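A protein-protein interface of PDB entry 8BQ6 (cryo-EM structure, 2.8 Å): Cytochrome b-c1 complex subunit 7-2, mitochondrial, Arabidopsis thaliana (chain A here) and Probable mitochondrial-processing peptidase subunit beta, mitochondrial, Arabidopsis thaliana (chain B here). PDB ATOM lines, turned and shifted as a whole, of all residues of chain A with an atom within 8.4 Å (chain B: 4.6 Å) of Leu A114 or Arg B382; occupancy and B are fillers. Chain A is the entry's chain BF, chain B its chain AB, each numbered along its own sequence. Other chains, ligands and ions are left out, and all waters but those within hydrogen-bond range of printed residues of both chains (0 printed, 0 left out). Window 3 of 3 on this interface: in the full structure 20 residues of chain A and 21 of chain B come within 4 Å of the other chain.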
ATOM      1  N   GLU A 104     -25.607  -0.887 -30.939  1.00  0.00           N
ATOM      2  CA  GLU A 104     -25.738  -0.774 -29.489  1.00  0.00           C
ATOM      3  C   GLU A 104     -25.018   0.460 -28.963  1.00  0.00           C
ATOM      4  O   GLU A 104     -25.492   1.113 -28.026  1.00  0.00           O
ATOM      5  CB  GLU A 104     -25.206  -2.034 -28.810  1.00  0.00           C
ATOM      6  CG  GLU A 104     -25.906  -3.307 -29.234  1.00  0.00           C
ATOM      7  CD  GLU A 104     -25.233  -4.539 -28.678  1.00  0.00           C
ATOM      8  OE1 GLU A 104     -24.311  -4.390 -27.849  1.00  0.00           O
ATOM      9  OE2 GLU A 104     -25.627  -5.656 -29.062  1.00  0.00           O
ATOM     10  N   ARG A 105     -23.864   0.785 -29.545  1.00  0.00           N
ATOM     11  CA  ARG A 105     -23.138   1.988 -29.151  1.00  0.00           C
ATOM     12  C   ARG A 105     -23.929   3.249 -29.485  1.00  0.00           C
ATOM     13  O   ARG A 105     -23.942   4.211 -28.708  1.00  0.00           O
ATOM     14  CB  ARG A 105     -21.767   2.001 -29.831  1.00  0.00           C
ATOM     15  CG  ARG A 105     -21.202   3.382 -30.105  1.00  0.00           C
ATOM     16  CD  ARG A 105     -20.290   3.374 -31.328  1.00  0.00           C
ATOM     17  NE  ARG A 105     -19.706   4.684 -31.593  1.00  0.00           N
ATOM     18  CZ  ARG A 105     -18.547   5.104 -31.102  1.00  0.00           C
ATOM     19  NH1 ARG A 105     -17.806   4.334 -30.323  1.00  0.00           N
ATOM     20  NH2 ARG A 105     -18.119   6.327 -31.406  1.00  0.00           N
ATOM     21  N   GLU A 107     -27.203   3.462 -29.743  1.00  0.00           N
ATOM     22  CA  GLU A 107     -28.359   3.504 -28.852  1.00  0.00           C
ATOM     23  C   GLU A 107     -27.980   4.041 -27.477  1.00  0.00           C
ATOM     24  O   GLU A 107     -28.723   4.832 -26.884  1.00  0.00           O
ATOM     25  CB  GLU A 107     -28.970   2.110 -28.736  1.00  0.00           C
ATOM     26  CG  GLU A 107     -30.148   2.015 -27.792  1.00  0.00           C
ATOM     27  CD  GLU A 107     -30.736   0.620 -27.756  1.00  0.00           C
ATOM     28  OE1 GLU A 107     -30.104  -0.278 -27.162  1.00  0.00           O
ATOM     29  OE2 GLU A 107     -31.830   0.420 -28.326  1.00  0.00           O
ATOM     30  N   ARG A 108     -26.829   3.615 -26.953  1.00  0.00           N
ATOM     31  CA  ARG A 108     -26.360   4.131 -25.672  1.00  0.00           C
ATOM     32  C   ARG A 108     -26.149   5.635 -25.729  1.00  0.00           C
ATOM     33  O   ARG A 108     -26.509   6.358 -24.793  1.00  0.00           O
ATOM     34  CB  ARG A 108     -25.056   3.445 -25.285  1.00  0.00           C
ATOM     35  CG  ARG A 108     -25.216   2.090 -24.670  1.00  0.00           C
ATOM     36  CD  ARG A 108     -23.899   1.683 -24.074  1.00  0.00           C
ATOM     37  NE  ARG A 108     -23.774   2.159 -22.705  1.00  0.00           N
ATOM     38  CZ  ARG A 108     -24.281   1.532 -21.655  1.00  0.00           C
ATOM     39  NH1 ARG A 108     -24.939   0.393 -21.786  1.00  0.00           N
ATOM     40  NH2 ARG A 108     -24.115   2.055 -20.445  1.00  0.00           N
ATOM     41  N   GLU A 109     -25.552   6.121 -26.816  1.00  0.00           N
ATOM     42  CA  GLU A 109     -25.289   7.548 -26.945  1.00  0.00           C
ATOM     43  C   GLU A 109     -26.582   8.349 -27.043  1.00  0.00           C
ATOM     44  O   GLU A 109     -26.697   9.424 -26.443  1.00  0.00           O
ATOM     45  CB  GLU A 109     -24.405   7.795 -28.165  1.00  0.00           C
ATOM     46  CG  GLU A 109     -23.816   9.181 -28.248  1.00  0.00           C
ATOM     47  CD  GLU A 109     -23.653   9.639 -29.680  1.00  0.00           C
ATOM     48  OE1 GLU A 109     -23.473  10.855 -29.903  1.00  0.00           O
ATOM     49  OE2 GLU A 109     -23.711   8.779 -30.585  1.00  0.00           O
ATOM     50  N   LEU A 111     -29.478   7.765 -25.792  1.00  0.00           N
ATOM     51  CA  LEU A 111     -30.227   7.767 -24.544  1.00  0.00           C
ATOM     52  C   LEU A 111     -29.444   8.367 -23.386  1.00  0.00           C
ATOM     53  O   LEU A 111     -29.877   8.250 -22.234  1.00  0.00           O
ATOM     54  CB  LEU A 111     -30.669   6.348 -24.192  1.00  0.00           C
ATOM     55  CG  LEU A 111     -31.844   5.842 -25.025  1.00  0.00           C
ATOM     56  CD1 LEU A 111     -32.207   4.424 -24.633  1.00  0.00           C
ATOM     57  CD2 LEU A 111     -33.031   6.767 -24.869  1.00  0.00           C
ATOM     58  N   GLY A 112     -28.299   8.986 -23.663  1.00  0.00           N
ATOM     59  CA  GLY A 112     -27.553   9.695 -22.645  1.00  0.00           C
ATOM     60  C   GLY A 112     -26.665   8.851 -21.763  1.00  0.00           C
ATOM     61  O   GLY A 112     -26.201   9.342 -20.732  1.00  0.00           O
ATOM     62  N   ALA A 113     -26.402   7.603 -22.132  1.00  0.00           N
ATOM     63  CA  ALA A 113     -25.612   6.724 -21.285  1.00  0.00           C
ATOM     64  C   ALA A 113     -24.121   6.880 -21.556  1.00  0.00           C
ATOM     65  O   ALA A 113     -23.697   7.404 -22.589  1.00  0.00           O
ATOM     66  CB  ALA A 113     -26.016   5.265 -21.485  1.00  0.00           C
ATOM     67  N   LEU A 114     -23.327   6.416 -20.594  1.00  0.00           N
ATOM     68  CA  LEU A 114     -21.887   6.359 -20.753  1.00  0.00           C
ATOM     69  C   LEU A 114     -21.510   5.254 -21.738  1.00  0.00           C
ATOM     70  O   LEU A 114     -22.229   4.262 -21.875  1.00  0.00           O
ATOM     71  CB  LEU A 114     -21.212   6.089 -19.411  1.00  0.00           C
ATOM     72  CG  LEU A 114     -21.300   7.141 -18.305  1.00  0.00           C
ATOM     73  CD1 LEU A 114     -20.725   6.583 -17.018  1.00  0.00           C
ATOM     74  CD2 LEU A 114     -20.571   8.406 -18.700  1.00  0.00           C
ATOM     75  N   PRO A 115     -20.390   5.406 -22.440  1.00  0.00           N
ATOM     76  CA  PRO A 115     -19.893   4.305 -23.271  1.00  0.00           C
ATOM     77  C   PRO A 115     -19.435   3.141 -22.408  1.00  0.00           C
ATOM     78  O   PRO A 115     -18.974   3.320 -21.280  1.00  0.00           O
ATOM     79  CB  PRO A 115     -18.719   4.931 -24.034  1.00  0.00           C
ATOM     80  CG  PRO A 115     -18.862   6.403 -23.855  1.00  0.00           C
ATOM     81  CD  PRO A 115     -19.550   6.607 -22.552  1.00  0.00           C
ATOM     82  N   LEU A 116     -19.568   1.932 -22.953  1.00  0.00           N
ATOM     83  CA  LEU A 116     -19.104   0.735 -22.264  1.00  0.00           C
ATOM     84  C   LEU A 116     -17.592   0.583 -22.296  1.00  0.00           C
ATOM     85  O   LEU A 116     -17.051  -0.248 -21.558  1.00  0.00           O
ATOM     86  CB  LEU A 116     -19.746  -0.509 -22.877  1.00  0.00           C
ATOM     87  CG  LEU A 116     -21.217  -0.737 -22.552  1.00  0.00           C
ATOM     88  CD1 LEU A 116     -21.723  -1.936 -23.318  1.00  0.00           C
ATOM     89  CD2 LEU A 116     -21.389  -0.943 -21.060  1.00  0.00           C
ATOM     90  N   TYR A 117     -16.909   1.348 -23.139  1.00  0.00           N
ATOM     91  CA  TYR A 117     -15.462   1.301 -23.281  1.00  0.00           C
ATOM     92  C   TYR A 117     -15.033   2.577 -23.983  1.00  0.00           C
ATOM     93  O   TYR A 117     -15.846   3.258 -24.616  1.00  0.00           O
ATOM     94  CB  TYR A 117     -15.010   0.065 -24.065  1.00  0.00           C
ATOM     95  CG  TYR A 117     -15.882  -0.237 -25.258  1.00  0.00           C
ATOM     96  CD1 TYR A 117     -15.709   0.438 -26.457  1.00  0.00           C
ATOM     97  CD2 TYR A 117     -16.891  -1.184 -25.180  1.00  0.00           C
ATOM     98  CE1 TYR A 117     -16.511   0.172 -27.545  1.00  0.00           C
ATOM     99  CE2 TYR A 117     -17.698  -1.456 -26.262  1.00  0.00           C
ATOM    100  CZ  TYR A 117     -17.502  -0.775 -27.441  1.00  0.00           C
ATOM    101  OH  TYR A 117     -18.304  -1.041 -28.525  1.00  0.00           O
ATOM    102  N   GLN A 118     -13.736   2.867 -23.920  1.00  0.00           N
ATOM    103  CA  GLN A 118     -13.169   4.088 -24.535  1.00  0.00           C
ATOM    104  C   GLN A 118     -11.727   3.779 -24.945  1.00  0.00           C
ATOM    105  O   GLN A 118     -11.150   2.813 -24.407  1.00  0.00           O
ATOM    106  CB  GLN A 118     -13.169   5.220 -23.512  1.00  0.00           C
ATOM    107  CG  GLN A 118     -14.312   6.209 -23.658  1.00  0.00           C
ATOM    108  CD  GLN A 118     -14.444   7.075 -22.430  1.00  0.00           C
ATOM    109  OE1 GLN A 118     -14.172   6.648 -21.312  1.00  0.00           O
ATOM    110  NE2 GLN A 118     -14.866   8.312 -22.632  1.00  0.00           N
ATOM    111  N   ASP B 378     -25.065   7.812 -13.556  1.00  0.00           N
ATOM    112  CA  ASP B 378     -23.724   7.758 -14.126  1.00  0.00           C
ATOM    113  C   ASP B 378     -22.715   7.199 -13.136  1.00  0.00           C
ATOM    114  O   ASP B 378     -21.720   6.592 -13.541  1.00  0.00           O
ATOM    115  CB  ASP B 378     -23.296   9.149 -14.580  1.00  0.00           C
ATOM    116  CG  ASP B 378     -24.047   9.614 -15.801  1.00  0.00           C
ATOM    117  OD1 ASP B 378     -24.687   8.776 -16.470  1.00  0.00           O
ATOM    118  OD2 ASP B 378     -24.000  10.826 -16.088  1.00  0.00           O
ATOM    119  N   LEU B 379     -22.938   7.420 -11.842  1.00  0.00           N
ATOM    120  CA  LEU B 379     -22.045   6.863 -10.835  1.00  0.00           C
ATOM    121  C   LEU B 379     -22.114   5.343 -10.823  1.00  0.00           C
ATOM    122  O   LEU B 379     -21.084   4.661 -10.784  1.00  0.00           O
ATOM    123  CB  LEU B 379     -22.396   7.432  -9.465  1.00  0.00           C
ATOM    124  CG  LEU B 379     -21.580   6.854  -8.318  1.00  0.00           C
ATOM    125  CD1 LEU B 379     -20.146   7.284  -8.472  1.00  0.00           C
ATOM    126  CD2 LEU B 379     -22.144   7.335  -7.005  1.00  0.00           C
ATOM    127  N   THR B 380     -23.329   4.794 -10.861  1.00  0.00           N
ATOM    128  CA  THR B 380     -23.487   3.345 -10.856  1.00  0.00           C
ATOM    129  C   THR B 380     -22.954   2.725 -12.140  1.00  0.00           C
ATOM    130  O   THR B 380     -22.434   1.602 -12.129  1.00  0.00           O
ATOM    131  CB  THR B 380     -24.958   2.990 -10.639  1.00  0.00           C
ATOM    132  OG1 THR B 380     -25.362   3.435  -9.339  1.00  0.00           O
ATOM    133  CG2 THR B 380     -25.183   1.497 -10.752  1.00  0.00           C
ATOM    134  N   GLN B 381     -23.066   3.440 -13.256  1.00  0.00           N
ATOM    135  CA  GLN B 381     -22.514   2.933 -14.506  1.00  0.00           C
ATOM    136  C   GLN B 381     -20.999   2.797 -14.418  1.00  0.00           C
ATOM    137  O   GLN B 381     -20.432   1.777 -14.824  1.00  0.00           O
ATOM    138  CB  GLN B 381     -22.908   3.849 -15.656  1.00  0.00           C
ATOM    139  CG  GLN B 381     -24.302   3.596 -16.160  1.00  0.00           C
ATOM    140  CD  GLN B 381     -24.693   4.575 -17.228  1.00  0.00           C
ATOM    141  OE1 GLN B 381     -24.540   4.307 -18.416  1.00  0.00           O
ATOM    142  NE2 GLN B 381     -25.182   5.734 -16.815  1.00  0.00           N
ATOM    143  N   ARG B 382     -20.326   3.810 -13.868  1.00  0.00           N
ATOM    144  CA  ARG B 382     -18.869   3.773 -13.786  1.00  0.00           C
ATOM    145  C   ARG B 382     -18.396   2.637 -12.888  1.00  0.00           C
ATOM    146  O   ARG B 382     -17.375   1.997 -13.162  1.00  0.00           O
ATOM    147  CB  ARG B 382     -18.335   5.113 -13.285  1.00  0.00           C
ATOM    148  CG  ARG B 382     -18.101   6.123 -14.387  1.00  0.00           C
ATOM    149  CD  ARG B 382     -17.740   7.484 -13.831  1.00  0.00           C
ATOM    150  NE  ARG B 382     -18.210   8.571 -14.681  1.00  0.00           N
ATOM    151  CZ  ARG B 382     -17.687   8.892 -15.858  1.00  0.00           C
ATOM    152  NH1 ARG B 382     -16.675   8.213 -16.375  1.00  0.00           N
ATOM    153  NH2 ARG B 382     -18.193   9.919 -16.534  1.00  0.00           N
ATOM    154  N   VAL B 383     -19.118   2.385 -11.797  1.00  0.00           N
ATOM    155  CA  VAL B 383     -18.742   1.301 -10.895  1.00  0.00           C
ATOM    156  C   VAL B 383     -19.028  -0.054 -11.532  1.00  0.00           C
ATOM    157  O   VAL B 383     -18.202  -0.973 -11.476  1.00  0.00           O
ATOM    158  CB  VAL B 383     -19.460   1.457  -9.544  1.00  0.00           C
ATOM    159  CG1 VAL B 383     -19.164   0.271  -8.660  1.00  0.00           C
ATOM    160  CG2 VAL B 383     -19.015   2.740  -8.869  1.00  0.00           C
ATOM    161  N   ALA B 384     -20.206  -0.205 -12.141  1.00  0.00           N
ATOM    162  CA  ALA B 384     -20.568  -1.500 -12.707  1.00  0.00           C
ATOM    163  C   ALA B 384     -19.767  -1.818 -13.961  1.00  0.00           C
ATOM    164  O   ALA B 384     -19.400  -2.978 -14.180  1.00  0.00           O
ATOM    165  CB  ALA B 384     -22.064  -1.547 -13.006  1.00  0.00           C
ATOM    166  N   ILE B 385     -19.486  -0.814 -14.794  1.00  0.00           N
ATOM    167  CA  ILE B 385     -18.780  -1.075 -16.044  1.00  0.00           C
ATOM    168  C   ILE B 385     -17.333  -1.472 -15.776  1.00  0.00           C
ATOM    169  O   ILE B 385     -16.802  -2.392 -16.408  1.00  0.00           O
ATOM    170  CB  ILE B 385     -18.879   0.147 -16.977  1.00  0.00           C
ATOM    171  CG1 ILE B 385     -20.197   0.109 -17.754  1.00  0.00           C
ATOM    172  CG2 ILE B 385     -17.716   0.185 -17.944  1.00  0.00           C
ATOM    173  CD1 ILE B 385     -20.705   1.467 -18.174  1.00  0.00           C
ATOM    174  N   ASN B 386     -16.677  -0.806 -14.830  1.00  0.00           N
ATOM    175  CA  ASN B 386     -15.259  -1.033 -14.584  1.00  0.00           C
ATOM    176  C   ASN B 386     -14.977  -1.947 -13.401  1.00  0.00           C
ATOM    177  O   ASN B 386     -13.805  -2.197 -13.106  1.00  0.00           O
ATOM    178  CB  ASN B 386     -14.544   0.300 -14.372  1.00  0.00           C
ATOM    179  CG  ASN B 386     -14.641   1.199 -15.573  1.00  0.00           C
ATOM    180  OD1 ASN B 386     -13.808   1.140 -16.473  1.00  0.00           O
ATOM    181  ND2 ASN B 386     -15.664   2.041 -15.600  1.00  0.00           N
ATOM    182  N   ILE B 388     -15.291  -1.624 -10.024  1.00  0.00           N
ATOM    183  CA  ILE B 388     -14.413  -0.921  -9.099  1.00  0.00           C
ATOM    184  C   ILE B 388     -14.984  -0.872  -7.681  1.00  0.00           C
ATOM    185  O   ILE B 388     -14.464  -0.151  -6.841  1.00  0.00           O
ATOM    186  CB  ILE B 388     -14.070   0.492  -9.611  1.00  0.00           C
ATOM    187  CG1 ILE B 388     -15.319   1.359  -9.735  1.00  0.00           C
ATOM    188  CG2 ILE B 388     -13.343   0.423 -10.940  1.00  0.00           C
ATOM    189  CD1 ILE B 388     -15.012   2.774 -10.144  1.00  0.00           C
ATOM    190  N   ALA B 422     -14.142   8.310  -9.040  1.00  0.00           N
ATOM    191  CA  ALA B 422     -15.466   8.195  -9.638  1.00  0.00           C
ATOM    192  C   ALA B 422     -16.527   8.841  -8.760  1.00  0.00           C
ATOM    193  O   ALA B 422     -17.398   9.564  -9.255  1.00  0.00           O
ATOM    194  CB  ALA B 422     -15.801   6.723  -9.877  1.00  0.00           C
ATOM    195  N   TYR B 425     -16.185  12.650  -8.827  1.00  0.00           N
ATOM    196  CA  TYR B 425     -16.501  13.216 -10.134  1.00  0.00           C
ATOM    197  C   TYR B 425     -18.006  13.336 -10.336  1.00  0.00           C
ATOM    198  O   TYR B 425     -18.498  14.350 -10.842  1.00  0.00           O
ATOM    199  CB  TYR B 425     -15.879  12.367 -11.242  1.00  0.00           C
ATOM    200  CG  TYR B 425     -16.065  12.964 -12.616  1.00  0.00           C
ATOM    201  CD1 TYR B 425     -15.131  13.841 -13.143  1.00  0.00           C
ATOM    202  CD2 TYR B 425     -17.184  12.664 -13.380  1.00  0.00           C
ATOM    203  CE1 TYR B 425     -15.299  14.392 -14.394  1.00  0.00           C
ATOM    204  CE2 TYR B 425     -17.363  13.213 -14.628  1.00  0.00           C
ATOM    205  CZ  TYR B 425     -16.417  14.074 -15.131  1.00  0.00           C
ATOM    206  OH  TYR B 425     -16.588  14.624 -16.377  1.00  0.00           O
ATOM    207  N   GLU B 426     -18.756  12.303  -9.950  1.00  0.00           N
ATOM    208  CA  GLU B 426     -20.191  12.310 -10.203  1.00  0.00           C
ATOM    209  C   GLU B 426     -20.942  13.181  -9.206  1.00  0.00           C
ATOM    210  O   GLU B 426     -21.997  13.730  -9.538  1.00  0.00           O
ATOM    211  CB  GLU B 426     -20.734  10.884 -10.182  1.00  0.00           C
ATOM    212  CG  GLU B 426     -20.207   9.996 -11.300  1.00  0.00           C
ATOM    213  CD  GLU B 426     -20.607  10.462 -12.694  1.00  0.00           C
ATOM    214  OE1 GLU B 426     -21.529  11.295 -12.828  1.00  0.00           O
ATOM    215  OE2 GLU B 426     -19.999   9.982 -13.671  1.00  0.00           O
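Leu A114 touches just these residues of chain B: Asp B378, Gln B381 and Arg B382.
Arg B382 touches one residue of chain A.
Of the printed residues of chain B, Arg A108 touches Gln B381 (3.1 Å).
Printed residues of chain B within 4 Å of Ala A113: Gln B381 (3.5 Å).
Printed residues of chain B within 4 Å of Leu A116: Ile B385.
Of the printed residues of chain A, Gln B381 touches Arg A108 (3.1 Å), Ala A113 (3.5 Å) and Leu A114 (3.3 Å).
Asn B386 touches none of the printed residues of chain A.
The nearest printed residue of chain B that does not touch Leu A114 is Ile B385 (4.8 Å).
The nearest residue of chain A that does not touch Arg B382 is Gln A118 (5.8 Å).
The nearest printed residue of chain B that does not touch Arg A108 is Ile B385 (4.1 Å).
Hydrophobic or aromatic side chains of chain A within 4 Å of the printed part of chain B: Ala A113, Leu A114 and Leu A116.
Of the 13 printed residues of chain B, 4 touch a printed residue of chain A.
Hydrophobic or aromatic side chains of chain B within 4 Å of the printed part of chain A: Ile B385.
Among the printed residues, 6 pairs touch across the chains.
Among the printed residues, no Asp or Glu carboxylate lies within 4 Å of a Lys or Arg side-chain nitrogen of the other chain.
Among the printed residues, pairs that only touch across the chains: Ala A113 with Gln B381 (3.5 Å), Leu A114 with Asp B378 (3.6 Å), Leu A114 with Arg B382 (3.6 Å) and Leu A116 with Ile B385 (3.7 Å).
The guanidinium group of Arg A108 sits at hydrogen-bond distance from the side-chain amide oxygen of Gln B381, 3.1 Å away.
The side-chain amide oxygen of Gln B381 is in hydrogen-bond range of the backbone NH of Leu A114 (3.3 Å).
OD1 of Asp B378 lies within hydrogen-bond range of NE2 of Gln B381 (3.1 Å).
The side-chain amide nitrogen of Asn B386 lies within hydrogen-bond range of the backbone carbonyl oxygen of Arg B382, at 3.0 Å.
The side-chain carboxylate of Glu B426 lies within salt-bridge range of the guanidinium group of Arg B382, 2.5 Å away.
The backbone carbonyl oxygen (O) of Arg A108 is in hydrogen-bond range of the backbone NH (N) of Ala A113 (2.9 Å).
The guanidinium group (NE) of Arg A108 lies within hydrogen-bond range of the backbone carbonyl oxygen (O) of Leu A114, at 2.7 Å.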
